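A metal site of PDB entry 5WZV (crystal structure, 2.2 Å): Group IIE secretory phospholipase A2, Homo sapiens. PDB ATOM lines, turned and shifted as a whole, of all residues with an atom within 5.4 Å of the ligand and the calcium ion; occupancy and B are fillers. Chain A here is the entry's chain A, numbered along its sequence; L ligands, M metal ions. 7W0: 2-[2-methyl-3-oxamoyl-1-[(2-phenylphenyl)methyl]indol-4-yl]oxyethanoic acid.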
ATOM      1  N   LEU A   2      29.203 -38.224  -6.821  1.00  0.00           N
ATOM      2  CA  LEU A   2      28.387 -37.001  -6.920  1.00  0.00           C
ATOM      3  C   LEU A   2      26.865 -37.213  -7.047  1.00  0.00           C
ATOM      4  O   LEU A   2      26.203 -36.485  -7.806  1.00  0.00           O
ATOM      5  CB  LEU A   2      28.899 -36.070  -8.041  1.00  0.00           C
ATOM      6  CG  LEU A   2      30.393 -35.858  -8.307  1.00  0.00           C
ATOM      7  CD1 LEU A   2      30.529 -35.215  -9.675  1.00  0.00           C
ATOM      8  CD2 LEU A   2      31.119 -35.038  -7.233  1.00  0.00           C
ATOM      9  N   VAL A   3      26.293 -38.165  -6.307  1.00  0.00           N
ATOM     10  CA  VAL A   3      24.829 -38.294  -6.275  1.00  0.00           C
ATOM     11  C   VAL A   3      24.200 -37.199  -5.400  1.00  0.00           C
ATOM     12  O   VAL A   3      23.148 -36.674  -5.753  1.00  0.00           O
ATOM     13  CB  VAL A   3      24.335 -39.748  -5.967  1.00  0.00           C
ATOM     14  CG1 VAL A   3      23.876 -39.927  -4.522  1.00  0.00           C
ATOM     15  CG2 VAL A   3      23.228 -40.142  -6.949  1.00  0.00           C
ATOM     16  N   PHE A   5      25.452 -34.064  -4.946  1.00  0.00           N
ATOM     17  CA  PHE A   5      25.502 -32.807  -5.766  1.00  0.00           C
ATOM     18  C   PHE A   5      24.377 -32.773  -6.816  1.00  0.00           C
ATOM     19  O   PHE A   5      23.660 -31.790  -6.938  1.00  0.00           O
ATOM     20  CB  PHE A   5      26.868 -32.614  -6.411  1.00  0.00           C
ATOM     21  CG  PHE A   5      27.032 -31.327  -7.203  1.00  0.00           C
ATOM     22  CD1 PHE A   5      26.377 -30.131  -6.843  1.00  0.00           C
ATOM     23  CD2 PHE A   5      27.825 -31.310  -8.330  1.00  0.00           C
ATOM     24  CE1 PHE A   5      26.543 -28.977  -7.577  1.00  0.00           C
ATOM     25  CE2 PHE A   5      28.004 -30.144  -9.069  1.00  0.00           C
ATOM     26  CZ  PHE A   5      27.362 -28.973  -8.696  1.00  0.00           C
ATOM     27  N   GLY A   6      24.214 -33.882  -7.549  1.00  0.00           N
ATOM     28  CA  GLY A   6      23.101 -34.067  -8.471  1.00  0.00           C
ATOM     29  C   GLY A   6      21.754 -33.865  -7.813  1.00  0.00           C
ATOM     30  O   GLY A   6      20.866 -33.216  -8.382  1.00  0.00           O
ATOM     31  N   ILE A   9      21.418 -30.130  -7.238  1.00  0.00           N
ATOM     32  CA  ILE A   9      21.076 -29.483  -8.508  1.00  0.00           C
ATOM     33  C   ILE A   9      19.579 -29.620  -8.812  1.00  0.00           C
ATOM     34  O   ILE A   9      18.884 -28.622  -9.071  1.00  0.00           O
ATOM     35  CB  ILE A   9      21.918 -30.042  -9.686  1.00  0.00           C
ATOM     36  CG1 ILE A   9      23.365 -29.558  -9.566  1.00  0.00           C
ATOM     37  CG2 ILE A   9      21.336 -29.606 -11.020  1.00  0.00           C
ATOM     38  CD1 ILE A   9      24.348 -30.399 -10.332  1.00  0.00           C
ATOM     39  N   ALA A  17      20.014 -33.448 -13.110  1.00  0.00           N
ATOM     40  CA  ALA A  17      21.475 -33.246 -13.113  1.00  0.00           C
ATOM     41  C   ALA A  17      22.126 -33.463 -14.477  1.00  0.00           C
ATOM     42  O   ALA A  17      23.145 -32.827 -14.781  1.00  0.00           O
ATOM     43  CB  ALA A  17      22.131 -34.151 -12.083  1.00  0.00           C
ATOM     44  N   LEU A  18      21.547 -34.379 -15.265  1.00  0.00           N
ATOM     45  CA  LEU A  18      21.932 -34.685 -16.661  1.00  0.00           C
ATOM     46  C   LEU A  18      22.021 -33.435 -17.533  1.00  0.00           C
ATOM     47  O   LEU A  18      22.838 -33.374 -18.441  1.00  0.00           O
ATOM     48  CB  LEU A  18      20.923 -35.630 -17.355  1.00  0.00           C
ATOM     49  CG  LEU A  18      20.411 -36.947 -16.728  1.00  0.00           C
ATOM     50  CD1 LEU A  18      19.387 -37.596 -17.649  1.00  0.00           C
ATOM     51  CD2 LEU A  18      21.528 -37.930 -16.376  1.00  0.00           C
ATOM     52  N   TYR A  20      23.062 -30.549 -16.732  1.00  0.00           N
ATOM     53  CA  TYR A  20      24.213 -29.723 -16.416  1.00  0.00           C
ATOM     54  C   TYR A  20      25.550 -30.395 -16.718  1.00  0.00           C
ATOM     55  O   TYR A  20      26.535 -29.698 -16.915  1.00  0.00           O
ATOM     56  CB  TYR A  20      24.133 -29.271 -14.959  1.00  0.00           C
ATOM     57  CG  TYR A  20      23.092 -28.197 -14.775  1.00  0.00           C
ATOM     58  CD1 TYR A  20      23.413 -26.863 -14.928  1.00  0.00           C
ATOM     59  CD2 TYR A  20      21.763 -28.521 -14.482  1.00  0.00           C
ATOM     60  CE1 TYR A  20      22.468 -25.869 -14.772  1.00  0.00           C
ATOM     61  CE2 TYR A  20      20.797 -27.537 -14.318  1.00  0.00           C
ATOM     62  CZ  TYR A  20      21.164 -26.206 -14.470  1.00  0.00           C
ATOM     63  OH  TYR A  20      20.237 -25.223 -14.318  1.00  0.00           O
ATOM     64  N   ASN A  21      25.587 -31.730 -16.780  1.00  0.00           N
ATOM     65  CA  ASN A  21      26.731 -32.439 -17.383  1.00  0.00           C
ATOM     66  C   ASN A  21      26.924 -32.038 -18.850  1.00  0.00           C
ATOM     67  O   ASN A  21      25.948 -31.848 -19.598  1.00  0.00           O
ATOM     68  CB  ASN A  21      26.520 -33.955 -17.299  1.00  0.00           C
ATOM     69  CG  ASN A  21      27.708 -34.744 -17.833  1.00  0.00           C
ATOM     70  OD1 ASN A  21      27.560 -35.580 -18.730  1.00  0.00           O
ATOM     71  ND2 ASN A  21      28.903 -34.473 -17.306  1.00  0.00           N
ATOM     72  N   TYR A  26      32.786 -25.871 -19.323  1.00  0.00           N
ATOM     73  CA  TYR A  26      33.244 -26.178 -17.970  1.00  0.00           C
ATOM     74  C   TYR A  26      32.381 -27.174 -17.195  1.00  0.00           C
ATOM     75  O   TYR A  26      32.884 -27.778 -16.264  1.00  0.00           O
ATOM     76  CB  TYR A  26      33.504 -24.892 -17.147  1.00  0.00           C
ATOM     77  CG  TYR A  26      34.771 -24.234 -17.620  1.00  0.00           C
ATOM     78  CD1 TYR A  26      36.009 -24.612 -17.106  1.00  0.00           C
ATOM     79  CD2 TYR A  26      34.755 -23.315 -18.668  1.00  0.00           C
ATOM     80  CE1 TYR A  26      37.210 -24.077 -17.589  1.00  0.00           C
ATOM     81  CE2 TYR A  26      35.941 -22.776 -19.159  1.00  0.00           C
ATOM     82  CZ  TYR A  26      37.173 -23.147 -18.616  1.00  0.00           C
ATOM     83  OH  TYR A  26      38.355 -22.629 -19.085  1.00  0.00           O
ATOM     84  N   CYS A  27      31.105 -27.339 -17.527  1.00  0.00           N
ATOM     85  CA  CYS A  27      30.282 -28.250 -16.734  1.00  0.00           C
ATOM     86  C   CYS A  27      30.487 -29.716 -17.181  1.00  0.00           C
ATOM     87  O   CYS A  27      30.233 -30.067 -18.333  1.00  0.00           O
ATOM     88  CB  CYS A  27      28.797 -27.877 -16.804  1.00  0.00           C
ATOM     89  SG  CYS A  27      28.347 -26.186 -16.382  1.00  0.00           S
ATOM     90  N   GLY A  28      30.897 -30.553 -16.249  1.00  0.00           N
ATOM     91  CA  GLY A  28      31.386 -31.901 -16.581  1.00  0.00           C
ATOM     92  C   GLY A  28      32.866 -31.919 -16.292  1.00  0.00           C
ATOM     93  O   GLY A  28      33.435 -30.882 -15.912  1.00  0.00           O
ATOM     94  N   ILE A  29      33.509 -33.069 -16.455  1.00  0.00           N
ATOM     95  CA  ILE A  29      34.894 -33.204 -15.977  1.00  0.00           C
ATOM     96  C   ILE A  29      35.863 -32.242 -16.691  1.00  0.00           C
ATOM     97  O   ILE A  29      35.767 -32.031 -17.914  1.00  0.00           O
ATOM     98  CB  ILE A  29      35.440 -34.657 -16.010  1.00  0.00           C
ATOM     99  CG1 ILE A  29      35.287 -35.305 -17.396  1.00  0.00           C
ATOM    100  CG2 ILE A  29      34.760 -35.490 -14.917  1.00  0.00           C
ATOM    101  CD1 ILE A  29      36.129 -36.558 -17.579  1.00  0.00           C
ATOM    102  N   GLY A  30      36.757 -31.645 -15.905  1.00  0.00           N
ATOM    103  CA  GLY A  30      37.696 -30.643 -16.390  1.00  0.00           C
ATOM    104  C   GLY A  30      36.995 -29.467 -17.051  1.00  0.00           C
ATOM    105  O   GLY A  30      35.994 -28.968 -16.529  1.00  0.00           O
ATOM    106  N   GLY A  31      37.495 -29.061 -18.208  1.00  0.00           N
ATOM    107  CA  GLY A  31      36.979 -27.904 -18.925  1.00  0.00           C
ATOM    108  C   GLY A  31      38.090 -26.920 -19.212  1.00  0.00           C
ATOM    109  O   GLY A  31      39.083 -26.880 -18.500  1.00  0.00           O
ATOM    110  N   CYS A  42      29.358 -20.592 -13.658  1.00  0.00           N
ATOM    111  CA  CYS A  42      29.117 -21.301 -12.399  1.00  0.00           C
ATOM    112  C   CYS A  42      30.014 -22.485 -12.271  1.00  0.00           C
ATOM    113  O   CYS A  42      30.598 -22.728 -11.221  1.00  0.00           O
ATOM    114  CB  CYS A  42      27.666 -21.772 -12.251  1.00  0.00           C
ATOM    115  SG  CYS A  42      26.382 -20.521 -12.372  1.00  0.00           S
ATOM    116  N   CYS A  43      30.123 -23.249 -13.360  1.00  0.00           N
ATOM    117  CA  CYS A  43      30.935 -24.451 -13.384  1.00  0.00           C
ATOM    118  C   CYS A  43      32.427 -24.165 -13.318  1.00  0.00           C
ATOM    119  O   CYS A  43      33.134 -24.851 -12.599  1.00  0.00           O
ATOM    120  CB  CYS A  43      30.600 -25.289 -14.603  1.00  0.00           C
ATOM    121  SG  CYS A  43      28.942 -25.982 -14.457  1.00  0.00           S
ATOM    122  N   HIS A  44      32.892 -23.151 -14.065  1.00  0.00           N
ATOM    123  CA  HIS A  44      34.242 -22.617 -13.952  1.00  0.00           C
ATOM    124  C   HIS A  44      34.602 -22.259 -12.501  1.00  0.00           C
ATOM    125  O   HIS A  44      35.668 -22.655 -11.999  1.00  0.00           O
ATOM    126  CB  HIS A  44      34.367 -21.360 -14.825  1.00  0.00           C
ATOM    127  CG  HIS A  44      35.725 -20.744 -14.791  1.00  0.00           C
ATOM    128  ND1 HIS A  44      36.084 -19.776 -13.876  1.00  0.00           N
ATOM    129  CD2 HIS A  44      36.818 -20.971 -15.548  1.00  0.00           C
ATOM    130  CE1 HIS A  44      37.341 -19.424 -14.080  1.00  0.00           C
ATOM    131  NE2 HIS A  44      37.802 -20.127 -15.097  1.00  0.00           N
ATOM    132  N   HIS A  46      33.048 -23.414  -9.840  1.00  0.00           N
ATOM    133  CA  HIS A  46      32.974 -24.671  -9.064  1.00  0.00           C
ATOM    134  C   HIS A  46      34.275 -25.459  -9.175  1.00  0.00           C
ATOM    135  O   HIS A  46      34.777 -25.950  -8.162  1.00  0.00           O
ATOM    136  CB  HIS A  46      31.802 -25.521  -9.542  1.00  0.00           C
ATOM    137  CG  HIS A  46      31.465 -26.679  -8.650  1.00  0.00           C
ATOM    138  ND1 HIS A  46      31.607 -27.988  -9.040  1.00  0.00           N
ATOM    139  CD2 HIS A  46      30.973 -26.720  -7.383  1.00  0.00           C
ATOM    140  CE1 HIS A  46      31.230 -28.784  -8.062  1.00  0.00           C
ATOM    141  NE2 HIS A  46      30.831 -28.037  -7.054  1.00  0.00           N
ATOM    142  N   ASP A  47      34.795 -25.578 -10.393  1.00  0.00           N
ATOM    143  CA  ASP A  47      36.118 -26.163 -10.627  1.00  0.00           C
ATOM    144  C   ASP A  47      37.209 -25.467  -9.813  1.00  0.00           C
ATOM    145  O   ASP A  47      38.085 -26.128  -9.240  1.00  0.00           O
ATOM    146  CB  ASP A  47      36.520 -26.027 -12.098  1.00  0.00           C
ATOM    147  CG  ASP A  47      35.769 -26.964 -13.002  1.00  0.00           C
ATOM    148  OD1 ASP A  47      34.848 -27.694 -12.547  1.00  0.00           O
ATOM    149  OD2 ASP A  47      36.104 -26.977 -14.198  1.00  0.00           O
ATOM    150  N   TYR A  50      36.766 -26.485  -6.108  1.00  0.00           N
ATOM    151  CA  TYR A  50      37.387 -27.792  -5.868  1.00  0.00           C
ATOM    152  C   TYR A  50      38.925 -27.727  -5.804  1.00  0.00           C
ATOM    153  O   TYR A  50      39.522 -28.364  -4.942  1.00  0.00           O
ATOM    154  CB  TYR A  50      36.895 -28.850  -6.866  1.00  0.00           C
ATOM    155  CG  TYR A  50      35.543 -29.520  -6.504  1.00  0.00           C
ATOM    156  CD1 TYR A  50      34.627 -28.917  -5.649  1.00  0.00           C
ATOM    157  CD2 TYR A  50      35.174 -30.733  -7.085  1.00  0.00           C
ATOM    158  CE1 TYR A  50      33.403 -29.542  -5.344  1.00  0.00           C
ATOM    159  CE2 TYR A  50      33.968 -31.361  -6.790  1.00  0.00           C
ATOM    160  CZ  TYR A  50      33.078 -30.772  -5.926  1.00  0.00           C
ATOM    161  OH  TYR A  50      31.880 -31.431  -5.624  1.00  0.00           O
ATOM    162  N   LYS A  61      36.112 -34.294  -5.024  1.00  0.00           N
ATOM    163  CA  LYS A  61      35.489 -35.229  -5.993  1.00  0.00           C
ATOM    164  C   LYS A  61      34.920 -36.477  -5.326  1.00  0.00           C
ATOM    165  O   LYS A  61      34.005 -37.072  -5.853  1.00  0.00           O
ATOM    166  CB  LYS A  61      36.493 -35.655  -7.073  1.00  0.00           C
ATOM    167  CG  LYS A  61      36.870 -34.560  -8.059  1.00  0.00           C
ATOM    168  CD  LYS A  61      37.778 -35.138  -9.130  1.00  0.00           C
ATOM    169  CE  LYS A  61      38.040 -34.164 -10.261  1.00  0.00           C
ATOM    170  NZ  LYS A  61      39.193 -33.297  -9.892  1.00  0.00           N
ATOM    171  N   ALA A  93      27.476 -23.324  -6.349  1.00  0.00           N
ATOM    172  CA  ALA A  93      27.170 -23.720  -7.729  1.00  0.00           C
ATOM    173  C   ALA A  93      25.698 -23.943  -8.020  1.00  0.00           C
ATOM    174  O   ALA A  93      25.197 -23.489  -9.015  1.00  0.00           O
ATOM    175  CB  ALA A  93      27.986 -24.966  -8.115  1.00  0.00           C
ATOM    176  N   PHE A  97      23.405 -21.907 -10.443  1.00  0.00           N
ATOM    177  CA  PHE A  97      22.550 -22.479 -11.510  1.00  0.00           C
ATOM    178  C   PHE A  97      21.136 -21.918 -11.434  1.00  0.00           C
ATOM    179  O   PHE A  97      20.613 -21.429 -12.444  1.00  0.00           O
ATOM    180  CB  PHE A  97      22.469 -24.009 -11.478  1.00  0.00           C
ATOM    181  CG  PHE A  97      23.750 -24.727 -11.760  1.00  0.00           C
ATOM    182  CD1 PHE A  97      24.738 -24.199 -12.616  1.00  0.00           C
ATOM    183  CD2 PHE A  97      23.981 -25.980 -11.194  1.00  0.00           C
ATOM    184  CE1 PHE A  97      25.917 -24.896 -12.859  1.00  0.00           C
ATOM    185  CE2 PHE A  97      25.156 -26.682 -11.443  1.00  0.00           C
ATOM    186  CZ  PHE A  97      26.120 -26.135 -12.285  1.00  0.00           C
HETATM  187  OAO 7W0 L   1      35.211 -31.311 -12.773  1.00  0.00           O
HETATM  188  CAN 7W0 L   1      35.073 -31.055 -11.542  1.00  0.00           C
HETATM  189  OAP 7W0 L   1      35.979 -30.709 -10.722  1.00  0.00           O
HETATM  190  CAM 7W0 L   1      33.632 -31.169 -10.959  1.00  0.00           C
HETATM  191  OAK 7W0 L   1      32.637 -30.963 -11.984  1.00  0.00           O
HETATM  192  CAA 7W0 L   1      31.826 -31.986 -12.431  1.00  0.00           C
HETATM  193  CAB 7W0 L   1      32.358 -33.285 -12.593  1.00  0.00           C
HETATM  194  CAC 7W0 L   1      31.531 -34.295 -13.054  1.00  0.00           C
HETATM  195  CAD 7W0 L   1      30.209 -33.965 -13.341  1.00  0.00           C
HETATM  196  CAE 7W0 L   1      29.726 -32.707 -13.179  1.00  0.00           C
HETATM  197  CAF 7W0 L   1      30.512 -31.700 -12.729  1.00  0.00           C
HETATM  198  CAI 7W0 L   1      29.729 -30.592 -12.702  1.00  0.00           C
HETATM  199  CAL 7W0 L   1      30.067 -29.335 -12.323  1.00  0.00           C
HETATM  200  OAS 7W0 L   1      29.438 -28.696 -11.463  1.00  0.00           O
HETATM  201  CAQ 7W0 L   1      31.269 -28.660 -13.009  1.00  0.00           C
HETATM  202  OAT 7W0 L   1      31.921 -29.216 -13.899  1.00  0.00           O
HETATM  203  NAR 7W0 L   1      31.602 -27.487 -12.520  1.00  0.00           N
HETATM  204  CAH 7W0 L   1      28.502 -30.932 -13.111  1.00  0.00           C
HETATM  205  CAJ 7W0 L   1      27.300 -29.976 -13.224  1.00  0.00           C
HETATM  206  NAG 7W0 L   1      28.483 -32.244 -13.413  1.00  0.00           N
HETATM  207  CAU 7W0 L   1      27.323 -33.089 -13.935  1.00  0.00           C
HETATM  208  CAV 7W0 L   1      26.729 -33.910 -12.900  1.00  0.00           C
HETATM  209  CAW 7W0 L   1      26.593 -33.374 -11.602  1.00  0.00           C
HETATM  210  CAX 7W0 L   1      26.036 -34.103 -10.554  1.00  0.00           C
HETATM  211  CAY 7W0 L   1      25.562 -35.379 -10.772  1.00  0.00           C
HETATM  212  CAZ 7W0 L   1      25.655 -35.936 -12.035  1.00  0.00           C
HETATM  213  CBA 7W0 L   1      26.216 -35.236 -13.106  1.00  0.00           C
HETATM  214  CBB 7W0 L   1      26.231 -35.989 -14.288  1.00  0.00           C
HETATM  215  CBC 7W0 L   1      27.392 -36.683 -14.673  1.00  0.00           C
HETATM  216  CBD 7W0 L   1      27.405 -37.466 -15.828  1.00  0.00           C
HETATM  217  CBE 7W0 L   1      26.255 -37.568 -16.615  1.00  0.00           C
HETATM  218  CBF 7W0 L   1      25.086 -36.894 -16.237  1.00  0.00           C
HETATM  219  CBG 7W0 L   1      25.071 -36.112 -15.065  1.00  0.00           C
HETATM  220 CA    CA M   1      34.176 -28.867 -14.841  1.00  0.00          CA
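The backbone carbonyl oxygen (O) of Cys 43 sits at hydrogen-bond distance from a nitrogen (NAR) of the ligand (3.0 Å).
A ring nitrogen (ND1) of His 46 sits at hydrogen-bond distance from an oxygen (OAS) of the ligand, at 3.3 Å.
The backbone NH of Gly 28 sits close to an oxygen (OAT) of the ligand.
NAR of the ligand lies close to SG of Cys 43 (3.6 Å).
The side-chain sulfur (SG) of Cys 43 forms a disulfide with the side-chain sulfur (SG) of Cys 27, at 2.0 Å.
Merely in contact with the ligand: Phe 5, Asn 21, Leu 2, Cys 27, Gly 6, Tyr 20, Leu 18, Tyr 50, Ile 29, Ala 17 and Ile 9.
Hydrophobic or aromatic side chains within 4 Å of the ligand: Leu 2, Phe 5, Ile 9, Ala 17, Leu 18, Tyr 20, Ile 29, His 46 and Tyr 50.
Within 4 Å of the ligand: Leu 2, Phe 5, Gly 6, Ile 9, Ala 17, Leu 18, Tyr 20, Asn 21, Tyr 26, Cys 27, Gly 28, Ile 29, Gly 30, Cys 43, His 46, Asp 47 and Tyr 50.
The nearest printed residue that does not touch the ligand is Lys 61 (4.05 Å).
Along chain A the residues within 4 Å of the calcium ion span positions 26 to 47.
The nearest printed residue that does not touch the calcium ion is Ile 29 (4.2 Å).
The calcium ion is bound by the backbone carbonyl oxygen (O) of Tyr 26, the backbone carbonyl oxygen (O) of Gly 28, an oxygen (OAT) of the ligand, the backbone carbonyl oxygen (O) of Gly 30, the side-chain carboxylate (OD1) of Asp 47 and the side-chain carboxylate (OD2) of Asp 47.
The calcium ion has six donor atoms within binding distance.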
